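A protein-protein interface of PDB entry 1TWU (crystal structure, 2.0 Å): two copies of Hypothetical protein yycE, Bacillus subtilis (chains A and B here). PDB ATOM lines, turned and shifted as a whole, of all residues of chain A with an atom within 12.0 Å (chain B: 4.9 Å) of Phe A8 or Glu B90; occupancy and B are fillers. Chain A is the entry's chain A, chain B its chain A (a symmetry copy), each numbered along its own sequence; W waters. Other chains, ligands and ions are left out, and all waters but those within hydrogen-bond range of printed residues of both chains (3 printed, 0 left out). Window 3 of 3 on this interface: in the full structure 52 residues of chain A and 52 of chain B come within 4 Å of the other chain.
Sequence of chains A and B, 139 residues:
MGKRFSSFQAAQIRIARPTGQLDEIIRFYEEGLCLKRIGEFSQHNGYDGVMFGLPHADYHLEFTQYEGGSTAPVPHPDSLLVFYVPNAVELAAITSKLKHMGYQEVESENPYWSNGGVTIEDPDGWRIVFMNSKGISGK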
ATOM      1  N   LYS A   3     -36.172  -2.511  25.343  1.00  0.00           N
ATOM      2  CA  LYS A   3     -35.380  -2.255  24.090  1.00  0.00           C
ATOM      3  C   LYS A   3     -34.985  -3.519  23.320  1.00  0.00           C
ATOM      4  O   LYS A   3     -33.811  -3.694  22.920  1.00  0.00           O
ATOM      5  CB  LYS A   3     -34.121  -1.431  24.408  1.00  0.00           C
ATOM      6  CG  LYS A   3     -33.177  -2.056  25.454  1.00  0.00           C
ATOM      7  CD  LYS A   3     -32.647  -0.972  26.425  1.00  0.00           C
ATOM      8  CE  LYS A   3     -31.912   0.143  25.680  1.00  0.00           C
ATOM      9  NZ  LYS A   3     -32.817   0.854  24.727  1.00  0.00           N
ATOM     10  N   ARG A   4     -35.961  -4.399  23.109  1.00  0.00           N
ATOM     11  CA  ARG A   4     -35.720  -5.615  22.352  1.00  0.00           C
ATOM     12  C   ARG A   4     -36.396  -5.439  20.996  1.00  0.00           C
ATOM     13  O   ARG A   4     -37.622  -5.504  20.893  1.00  0.00           O
ATOM     14  CB  ARG A   4     -36.311  -6.826  23.067  1.00  0.00           C
ATOM     15  CG  ARG A   4     -35.733  -8.146  22.585  1.00  0.00           C
ATOM     16  CD  ARG A   4     -36.361  -9.312  23.327  1.00  0.00           C
ATOM     17  NE  ARG A   4     -37.576  -9.793  22.673  1.00  0.00           N
ATOM     18  CZ  ARG A   4     -38.585 -10.385  23.307  1.00  0.00           C
ATOM     19  NH1 ARG A   4     -38.534 -10.565  24.622  1.00  0.00           N
ATOM     20  NH2 ARG A   4     -39.645 -10.812  22.625  1.00  0.00           N
ATOM     21  N   PHE A   5     -35.594  -5.190  19.963  1.00  0.00           N
ATOM     22  CA  PHE A   5     -36.124  -5.015  18.616  1.00  0.00           C
ATOM     23  C   PHE A   5     -36.329  -6.383  17.971  1.00  0.00           C
ATOM     24  O   PHE A   5     -35.786  -7.386  18.438  1.00  0.00           O
ATOM     25  CB  PHE A   5     -35.161  -4.172  17.767  1.00  0.00           C
ATOM     26  CG  PHE A   5     -35.074  -2.730  18.193  1.00  0.00           C
ATOM     27  CD1 PHE A   5     -34.550  -2.384  19.436  1.00  0.00           C
ATOM     28  CD2 PHE A   5     -35.547  -1.717  17.360  1.00  0.00           C
ATOM     29  CE1 PHE A   5     -34.503  -1.049  19.846  1.00  0.00           C
ATOM     30  CE2 PHE A   5     -35.505  -0.380  17.759  1.00  0.00           C
ATOM     31  CZ  PHE A   5     -34.983  -0.046  19.004  1.00  0.00           C
ATOM     32  N   SER A   6     -37.114  -6.419  16.899  1.00  0.00           N
ATOM     33  CA  SER A   6     -37.397  -7.666  16.192  1.00  0.00           C
ATOM     34  C   SER A   6     -36.155  -8.266  15.532  1.00  0.00           C
ATOM     35  O   SER A   6     -35.942  -9.477  15.575  1.00  0.00           O
ATOM     36  CB  SER A   6     -38.461  -7.430  15.117  1.00  0.00           C
ATOM     37  OG  SER A   6     -39.649  -6.905  15.675  1.00  0.00           O
ATOM     38  N   SER A   7     -35.339  -7.409  14.928  1.00  0.00           N
ATOM     39  CA  SER A   7     -34.141  -7.851  14.232  1.00  0.00           C
ATOM     40  C   SER A   7     -32.890  -7.936  15.097  1.00  0.00           C
ATOM     41  O   SER A   7     -31.903  -8.543  14.692  1.00  0.00           O
ATOM     42  CB  SER A   7     -33.863  -6.918  13.050  1.00  0.00           C
ATOM     43  OG  SER A   7     -34.977  -6.854  12.178  1.00  0.00           O
ATOM     44  N   PHE A   8     -32.917  -7.340  16.283  1.00  0.00           N
ATOM     45  CA  PHE A   8     -31.731  -7.363  17.130  1.00  0.00           C
ATOM     46  C   PHE A   8     -31.957  -6.798  18.517  1.00  0.00           C
ATOM     47  O   PHE A   8     -32.975  -6.167  18.797  1.00  0.00           O
ATOM     48  CB  PHE A   8     -30.617  -6.571  16.454  1.00  0.00           C
ATOM     49  CG  PHE A   8     -31.011  -5.163  16.110  1.00  0.00           C
ATOM     50  CD1 PHE A   8     -31.017  -4.170  17.083  1.00  0.00           C
ATOM     51  CD2 PHE A   8     -31.420  -4.839  14.820  1.00  0.00           C
ATOM     52  CE1 PHE A   8     -31.422  -2.874  16.778  1.00  0.00           C
ATOM     53  CE2 PHE A   8     -31.827  -3.548  14.506  1.00  0.00           C
ATOM     54  CZ  PHE A   8     -31.829  -2.565  15.488  1.00  0.00           C
ATOM     55  N   GLN A   9     -30.983  -7.025  19.385  1.00  0.00           N
ATOM     56  CA  GLN A   9     -31.050  -6.532  20.750  1.00  0.00           C
ATOM     57  C   GLN A   9     -30.204  -5.266  20.825  1.00  0.00           C
ATOM     58  O   GLN A   9     -28.988  -5.304  20.623  1.00  0.00           O
ATOM     59  CB  GLN A   9     -30.517  -7.597  21.723  1.00  0.00           C
ATOM     60  CG  GLN A   9     -30.506  -7.179  23.198  1.00  0.00           C
ATOM     61  CD  GLN A   9     -31.889  -6.822  23.722  1.00  0.00           C
ATOM     62  OE1 GLN A   9     -32.843  -7.586  23.551  1.00  0.00           O
ATOM     63  NE2 GLN A   9     -32.003  -5.660  24.371  1.00  0.00           N
ATOM     64  N   ALA A  10     -30.855  -4.141  21.095  1.00  0.00           N
ATOM     65  CA  ALA A  10     -30.150  -2.871  21.197  1.00  0.00           C
ATOM     66  C   ALA A  10     -29.832  -2.576  22.649  1.00  0.00           C
ATOM     67  O   ALA A  10     -30.716  -2.593  23.501  1.00  0.00           O
ATOM     68  CB  ALA A  10     -30.995  -1.745  20.612  1.00  0.00           C
ATOM     69  N   ALA A  11     -28.564  -2.314  22.931  1.00  0.00           N
ATOM     70  CA  ALA A  11     -28.144  -1.993  24.285  1.00  0.00           C
ATOM     71  C   ALA A  11     -28.467  -0.527  24.585  1.00  0.00           C
ATOM     72  O   ALA A  11     -28.880  -0.172  25.692  1.00  0.00           O
ATOM     73  CB  ALA A  11     -26.647  -2.237  24.432  1.00  0.00           C
ATOM     74  N   GLN A  12     -28.312   0.317  23.574  1.00  0.00           N
ATOM     75  CA  GLN A  12     -28.529   1.745  23.743  1.00  0.00           C
ATOM     76  C   GLN A  12     -28.901   2.367  22.408  1.00  0.00           C
ATOM     77  O   GLN A  12     -28.735   1.741  21.365  1.00  0.00           O
ATOM     78  CB  GLN A  12     -27.228   2.371  24.230  1.00  0.00           C
ATOM     79  CG  GLN A  12     -27.342   3.260  25.419  1.00  0.00           C
ATOM     80  CD  GLN A  12     -25.981   3.637  25.963  1.00  0.00           C
ATOM     81  OE1 GLN A  12     -25.154   4.231  25.262  1.00  0.00           O
ATOM     82  NE2 GLN A  12     -25.737   3.289  27.220  1.00  0.00           N
ATOM     83  N   ILE A  13     -29.401   3.596  22.449  1.00  0.00           N
ATOM     84  CA  ILE A  13     -29.757   4.320  21.234  1.00  0.00           C
ATOM     85  C   ILE A  13     -29.306   5.767  21.385  1.00  0.00           C
ATOM     86  O   ILE A  13     -29.541   6.404  22.418  1.00  0.00           O
ATOM     87  CB  ILE A  13     -31.275   4.281  20.945  1.00  0.00           C
ATOM     88  CG1 ILE A  13     -31.710   2.842  20.688  1.00  0.00           C
ATOM     89  CG2 ILE A  13     -31.597   5.122  19.705  1.00  0.00           C
ATOM     90  CD1 ILE A  13     -33.167   2.710  20.348  1.00  0.00           C
ATOM     91  N   ARG A  14     -28.643   6.268  20.349  1.00  0.00           N
ATOM     92  CA  ARG A  14     -28.128   7.624  20.341  1.00  0.00           C
ATOM     93  C   ARG A  14     -28.539   8.416  19.105  1.00  0.00           C
ATOM     94  O   ARG A  14     -28.507   7.904  17.984  1.00  0.00           O
ATOM     95  CB  ARG A  14     -26.596   7.600  20.427  1.00  0.00           C
ATOM     96  CG  ARG A  14     -25.940   8.967  20.228  1.00  0.00           C
ATOM     97  CD  ARG A  14     -24.424   8.891  20.210  1.00  0.00           C
ATOM     98  NE  ARG A  14     -23.876   8.552  21.522  1.00  0.00           N
ATOM     99  CZ  ARG A  14     -22.580   8.398  21.788  1.00  0.00           C
ATOM    100  NH1 ARG A  14     -21.677   8.552  20.831  1.00  0.00           N
ATOM    101  NH2 ARG A  14     -22.185   8.088  23.016  1.00  0.00           N
ATOM    102  N   ASP A  58     -29.783   4.876  28.134  1.00  0.00           N
ATOM    103  CA  ASP A  58     -30.462   3.987  27.190  1.00  0.00           C
ATOM    104  C   ASP A  58     -30.815   4.729  25.912  1.00  0.00           C
ATOM    105  O   ASP A  58     -30.633   4.215  24.812  1.00  0.00           O
ATOM    106  CB  ASP A  58     -31.733   3.405  27.807  1.00  0.00           C
ATOM    107  CG  ASP A  58     -31.438   2.444  28.945  1.00  0.00           C
ATOM    108  OD1 ASP A  58     -30.341   1.839  28.947  1.00  0.00           O
ATOM    109  OD2 ASP A  58     -32.306   2.280  29.829  1.00  0.00           O
ATOM    110  N   TYR A  59     -31.342   5.935  26.081  1.00  0.00           N
ATOM    111  CA  TYR A  59     -31.712   6.805  24.976  1.00  0.00           C
ATOM    112  C   TYR A  59     -31.103   8.152  25.319  1.00  0.00           C
ATOM    113  O   TYR A  59     -31.476   8.766  26.317  1.00  0.00           O
ATOM    114  CB  TYR A  59     -33.232   6.959  24.865  1.00  0.00           C
ATOM    115  CG  TYR A  59     -33.968   5.691  24.497  1.00  0.00           C
ATOM    116  CD1 TYR A  59     -34.361   4.775  25.477  1.00  0.00           C
ATOM    117  CD2 TYR A  59     -34.260   5.396  23.161  1.00  0.00           C
ATOM    118  CE1 TYR A  59     -35.027   3.600  25.132  1.00  0.00           C
ATOM    119  CE2 TYR A  59     -34.923   4.226  22.806  1.00  0.00           C
ATOM    120  CZ  TYR A  59     -35.303   3.332  23.794  1.00  0.00           C
ATOM    121  OH  TYR A  59     -35.948   2.163  23.437  1.00  0.00           O
ATOM    122  N   LEU B  33     -35.474  -2.602   8.774  1.00  0.00           N
ATOM    123  CA  LEU B  33     -35.170  -2.717  10.195  1.00  0.00           C
ATOM    124  C   LEU B  33     -36.170  -3.569  10.946  1.00  0.00           C
ATOM    125  O   LEU B  33     -35.868  -4.080  12.022  1.00  0.00           O
ATOM    126  CB  LEU B  33     -35.130  -1.340  10.849  1.00  0.00           C
ATOM    127  CG  LEU B  33     -33.898  -0.506  10.530  1.00  0.00           C
ATOM    128  CD1 LEU B  33     -33.958   0.808  11.304  1.00  0.00           C
ATOM    129  CD2 LEU B  33     -32.655  -1.303  10.906  1.00  0.00           C
ATOM    130  N   PHE B  83     -27.452   2.651  16.753  1.00  0.00           N
ATOM    131  CA  PHE B  83     -27.983   1.466  17.408  1.00  0.00           C
ATOM    132  C   PHE B  83     -26.779   0.714  17.963  1.00  0.00           C
ATOM    133  O   PHE B  83     -25.917   0.289  17.196  1.00  0.00           O
ATOM    134  CB  PHE B  83     -28.700   0.569  16.401  1.00  0.00           C
ATOM    135  CG  PHE B  83     -30.069   1.054  16.005  1.00  0.00           C
ATOM    136  CD1 PHE B  83     -31.132   0.993  16.905  1.00  0.00           C
ATOM    137  CD2 PHE B  83     -30.303   1.545  14.720  1.00  0.00           C
ATOM    138  CE1 PHE B  83     -32.409   1.407  16.529  1.00  0.00           C
ATOM    139  CE2 PHE B  83     -31.576   1.965  14.336  1.00  0.00           C
ATOM    140  CZ  PHE B  83     -32.632   1.895  15.242  1.00  0.00           C
ATOM    141  N   VAL B  85     -25.426  -2.431  19.066  1.00  0.00           N
ATOM    142  CA  VAL B  85     -25.746  -3.850  19.000  1.00  0.00           C
ATOM    143  C   VAL B  85     -24.547  -4.676  19.428  1.00  0.00           C
ATOM    144  O   VAL B  85     -23.716  -5.053  18.605  1.00  0.00           O
ATOM    145  CB  VAL B  85     -26.138  -4.271  17.578  1.00  0.00           C
ATOM    146  CG1 VAL B  85     -26.725  -5.670  17.606  1.00  0.00           C
ATOM    147  CG2 VAL B  85     -27.124  -3.284  16.994  1.00  0.00           C
ATOM    148  N   ASN B  87     -24.171  -7.783  20.157  1.00  0.00           N
ATOM    149  CA  ASN B  87     -24.061  -9.097  19.528  1.00  0.00           C
ATOM    150  C   ASN B  87     -23.653  -8.933  18.067  1.00  0.00           C
ATOM    151  O   ASN B  87     -24.494  -8.657  17.213  1.00  0.00           O
ATOM    152  CB  ASN B  87     -25.396  -9.832  19.589  1.00  0.00           C
ATOM    153  CG  ASN B  87     -25.290 -11.278  19.115  1.00  0.00           C
ATOM    154  OD1 ASN B  87     -24.561 -11.589  18.169  1.00  0.00           O
ATOM    155  ND2 ASN B  87     -26.036 -12.164  19.764  1.00  0.00           N
ATOM    156  N   ALA B  88     -22.365  -9.124  17.791  1.00  0.00           N
ATOM    157  CA  ALA B  88     -21.813  -8.977  16.446  1.00  0.00           C
ATOM    158  C   ALA B  88     -22.508  -9.784  15.354  1.00  0.00           C
ATOM    159  O   ALA B  88     -22.508  -9.377  14.190  1.00  0.00           O
ATOM    160  CB  ALA B  88     -20.332  -9.305  16.461  1.00  0.00           C
ATOM    161  N   VAL B  89     -23.091 -10.925  15.717  1.00  0.00           N
ATOM    162  CA  VAL B  89     -23.791 -11.760  14.743  1.00  0.00           C
ATOM    163  C   VAL B  89     -25.081 -11.083  14.293  1.00  0.00           C
ATOM    164  O   VAL B  89     -25.408 -11.097  13.107  1.00  0.00           O
ATOM    165  CB  VAL B  89     -24.123 -13.161  15.322  1.00  0.00           C
ATOM    166  CG1 VAL B  89     -25.054 -13.925  14.377  1.00  0.00           C
ATOM    167  CG2 VAL B  89     -22.833 -13.944  15.535  1.00  0.00           C
ATOM    168  N   GLU B  90     -25.816 -10.497  15.235  1.00  0.00           N
ATOM    169  CA  GLU B  90     -27.054  -9.803  14.892  1.00  0.00           C
ATOM    170  C   GLU B  90     -26.716  -8.552  14.091  1.00  0.00           C
ATOM    171  O   GLU B  90     -27.403  -8.210  13.131  1.00  0.00           O
ATOM    172  CB  GLU B  90     -27.814  -9.392  16.145  1.00  0.00           C
ATOM    173  CG  GLU B  90     -28.203 -10.531  17.033  1.00  0.00           C
ATOM    174  CD  GLU B  90     -28.987 -10.056  18.219  1.00  0.00           C
ATOM    175  OE1 GLU B  90     -28.654  -8.971  18.745  1.00  0.00           O
ATOM    176  OE2 GLU B  90     -29.929 -10.764  18.631  1.00  0.00           O
ATOM    177  N   LEU B  91     -25.657  -7.862  14.499  1.00  0.00           N
ATOM    178  CA  LEU B  91     -25.235  -6.658  13.800  1.00  0.00           C
ATOM    179  C   LEU B  91     -24.970  -7.023  12.336  1.00  0.00           C
ATOM    180  O   LEU B  91     -25.537  -6.420  11.427  1.00  0.00           O
ATOM    181  CB  LEU B  91     -23.976  -6.083  14.462  1.00  0.00           C
ATOM    182  CG  LEU B  91     -23.544  -4.655  14.113  1.00  0.00           C
ATOM    183  CD1 LEU B  91     -22.600  -4.145  15.188  1.00  0.00           C
ATOM    184  CD2 LEU B  91     -22.884  -4.606  12.747  1.00  0.00           C
ATOM    185  N   ALA B  92     -24.130  -8.030  12.112  1.00  0.00           N
ATOM    186  CA  ALA B  92     -23.800  -8.467  10.758  1.00  0.00           C
ATOM    187  C   ALA B  92     -25.046  -8.836   9.955  1.00  0.00           C
ATOM    188  O   ALA B  92     -25.148  -8.519   8.767  1.00  0.00           O
ATOM    189  CB  ALA B  92     -22.849  -9.657  10.808  1.00  0.00           C
ATOM    190  N   ALA B  93     -25.991  -9.506  10.609  1.00  0.00           N
ATOM    191  CA  ALA B  93     -27.223  -9.934   9.960  1.00  0.00           C
ATOM    192  C   ALA B  93     -28.104  -8.787   9.486  1.00  0.00           C
ATOM    193  O   ALA B  93     -28.580  -8.794   8.353  1.00  0.00           O
ATOM    194  CB  ALA B  93     -28.018 -10.824  10.896  1.00  0.00           C
ATOM    195  N   ILE B  94     -28.329  -7.802  10.350  1.00  0.00           N
ATOM    196  CA  ILE B  94     -29.184  -6.689   9.970  1.00  0.00           C
ATOM    197  C   ILE B  94     -28.555  -5.820   8.879  1.00  0.00           C
ATOM    198  O   ILE B  94     -29.212  -5.492   7.884  1.00  0.00           O
ATOM    199  CB  ILE B  94     -29.577  -5.813  11.203  1.00  0.00           C
ATOM    200  CG1 ILE B  94     -30.581  -4.740  10.769  1.00  0.00           C
ATOM    201  CG2 ILE B  94     -28.349  -5.155  11.819  1.00  0.00           C
ATOM    202  CD1 ILE B  94     -31.808  -5.298  10.057  1.00  0.00           C
ATOM    203  N   PHE B 130     -24.670   1.143  13.256  1.00  0.00           N
ATOM    204  CA  PHE B 130     -24.789  -0.051  14.078  1.00  0.00           C
ATOM    205  C   PHE B 130     -23.400  -0.241  14.695  1.00  0.00           C
ATOM    206  O   PHE B 130     -22.450  -0.638  14.014  1.00  0.00           O
ATOM    207  CB  PHE B 130     -25.195  -1.233  13.198  1.00  0.00           C
ATOM    208  CG  PHE B 130     -26.520  -1.038  12.521  1.00  0.00           C
ATOM    209  CD1 PHE B 130     -27.702  -1.435  13.143  1.00  0.00           C
ATOM    210  CD2 PHE B 130     -26.595  -0.397  11.287  1.00  0.00           C
ATOM    211  CE1 PHE B 130     -28.946  -1.196  12.549  1.00  0.00           C
ATOM    212  CE2 PHE B 130     -27.827  -0.152  10.684  1.00  0.00           C
ATOM    213  CZ  PHE B 130     -29.007  -0.551  11.317  1.00  0.00           C
HETATM  214  O   HOH W   1     -27.084  -7.386  20.378  1.00  0.00           O
HETATM  215  O   HOH W   2     -29.813  -9.082  13.407  1.00  0.00           O
HETATM  216  O   HOH W   3     -36.070  -4.465  14.935  1.00  0.00           O
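Water W2 bridges O of Ser A7 (2.5 Å) and O of Glu B90 (2.6 Å).
Water W1 lies within hydrogen-bond range of the side-chain carboxylate of Glu B90 (2.8 Å), the backbone carbonyl oxygen of Gln A9 (2.8 Å) and the backbone NH of Asn B87 (2.9 Å).
Water W3 lies within hydrogen-bond range of the backbone carbonyl oxygen of Leu B33 (2.9 Å), the backbone NH of Ser A6 (3.0 Å) and the backbone NH of Ser A7 (3.0 Å).
No position is printed for both chains.
Of the 8 pairs that touch across the chains among the printed residues, none has its exchanged pair printed and touching as well.
Printed residues of chain B within 4 Å of Phe A5: Phe B83.
Printed residues of chain B within 4 Å of Ser A7: Leu B33 and Ile B94.
Of the printed residues of chain B, Phe A8 touches Phe B83 (3.9 Å), Val B85 (3.99 Å) and Glu B90 (3.8 Å).
Of the printed residues of chain B, Gln A9 touches Val B85 (3.8 Å) and Glu B90 (3.1 Å).
Leu B33 touches one residue of chain A.
Phe B83 touches two residues of chain A.
Of the printed residues of chain A, Val B85 touches Phe A8 (3.99 Å) and Gln A9 (3.8 Å).
No residue of chain A comes within 4 Å of Asn B87.
No residue of chain A comes within 4 Å of Val B89.
Glu B90 touches just these residues of chain A: Phe A8 (3.8 Å) and Gln A9 (3.1 Å).
No residue of chain A comes within 4 Å of Leu B91.
Ala B92 touches none of the printed residues of chain A.
No residue of chain A comes within 4 Å of Ala B93.
Ile B94 touches just one residue of chain A: Ser A7.
The nearest printed residue of chain B that does not touch Phe A8 is Ile B94 (4.1 Å).
The nearest residue of chain A that does not touch Glu B90 is Ser A7 (4.4 Å).
The nearest printed residue of chain B that does not touch Phe A5 is Leu B33 (5.8 Å).
The backbone NH (N) of Gln A9 is in hydrogen-bond range of the side-chain carboxylate (OE1) of Glu B90, 3.1 Å away.
The side-chain hydroxyl of Ser A7 is in hydrogen-bond range of the backbone carbonyl oxygen of Leu B33, at 2.9 Å.
Hydrophobic or aromatic side chains of chain A within 4 Å of the printed part of chain B: Phe A5 and Phe A8.
Printed residues of chain B that touch a printed residue of chain A: Leu B33, Phe B83, Val B85, Glu B90 and Ile B94.
Hydrophobic or aromatic side chains of chain B within 4 Å of the printed part of chain A: Phe B83, Val B85 and Ile B94.
Among the printed residues, no Asp or Glu carboxylate lies within 4 Å of a Lys or Arg side-chain nitrogen of the other chain.
The side-chain amide nitrogen (NE2) of Gln A9 sits at hydrogen-bond distance from the backbone carbonyl oxygen (O) of Lys A3.
OD1 of Asn B87 is in hydrogen-bond range of N of Glu B90 (3.4 Å).
CE1 of Phe B83 touches CE2 of Phe A5, 3.8 Å away.
Ser A7 touches Ile B94 (CB to CD1, 3.98 Å).
CE1 of Phe A8 touches CD1 of Phe B83 (3.9 Å).
Phe A8 touches Val B85 (CD1 to CG2, 3.99 Å).
OE1 of Glu B90 touches CA of Phe A8 (3.8 Å).
O of Gln A9 touches CG1 of Val B85, at 3.8 Å.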
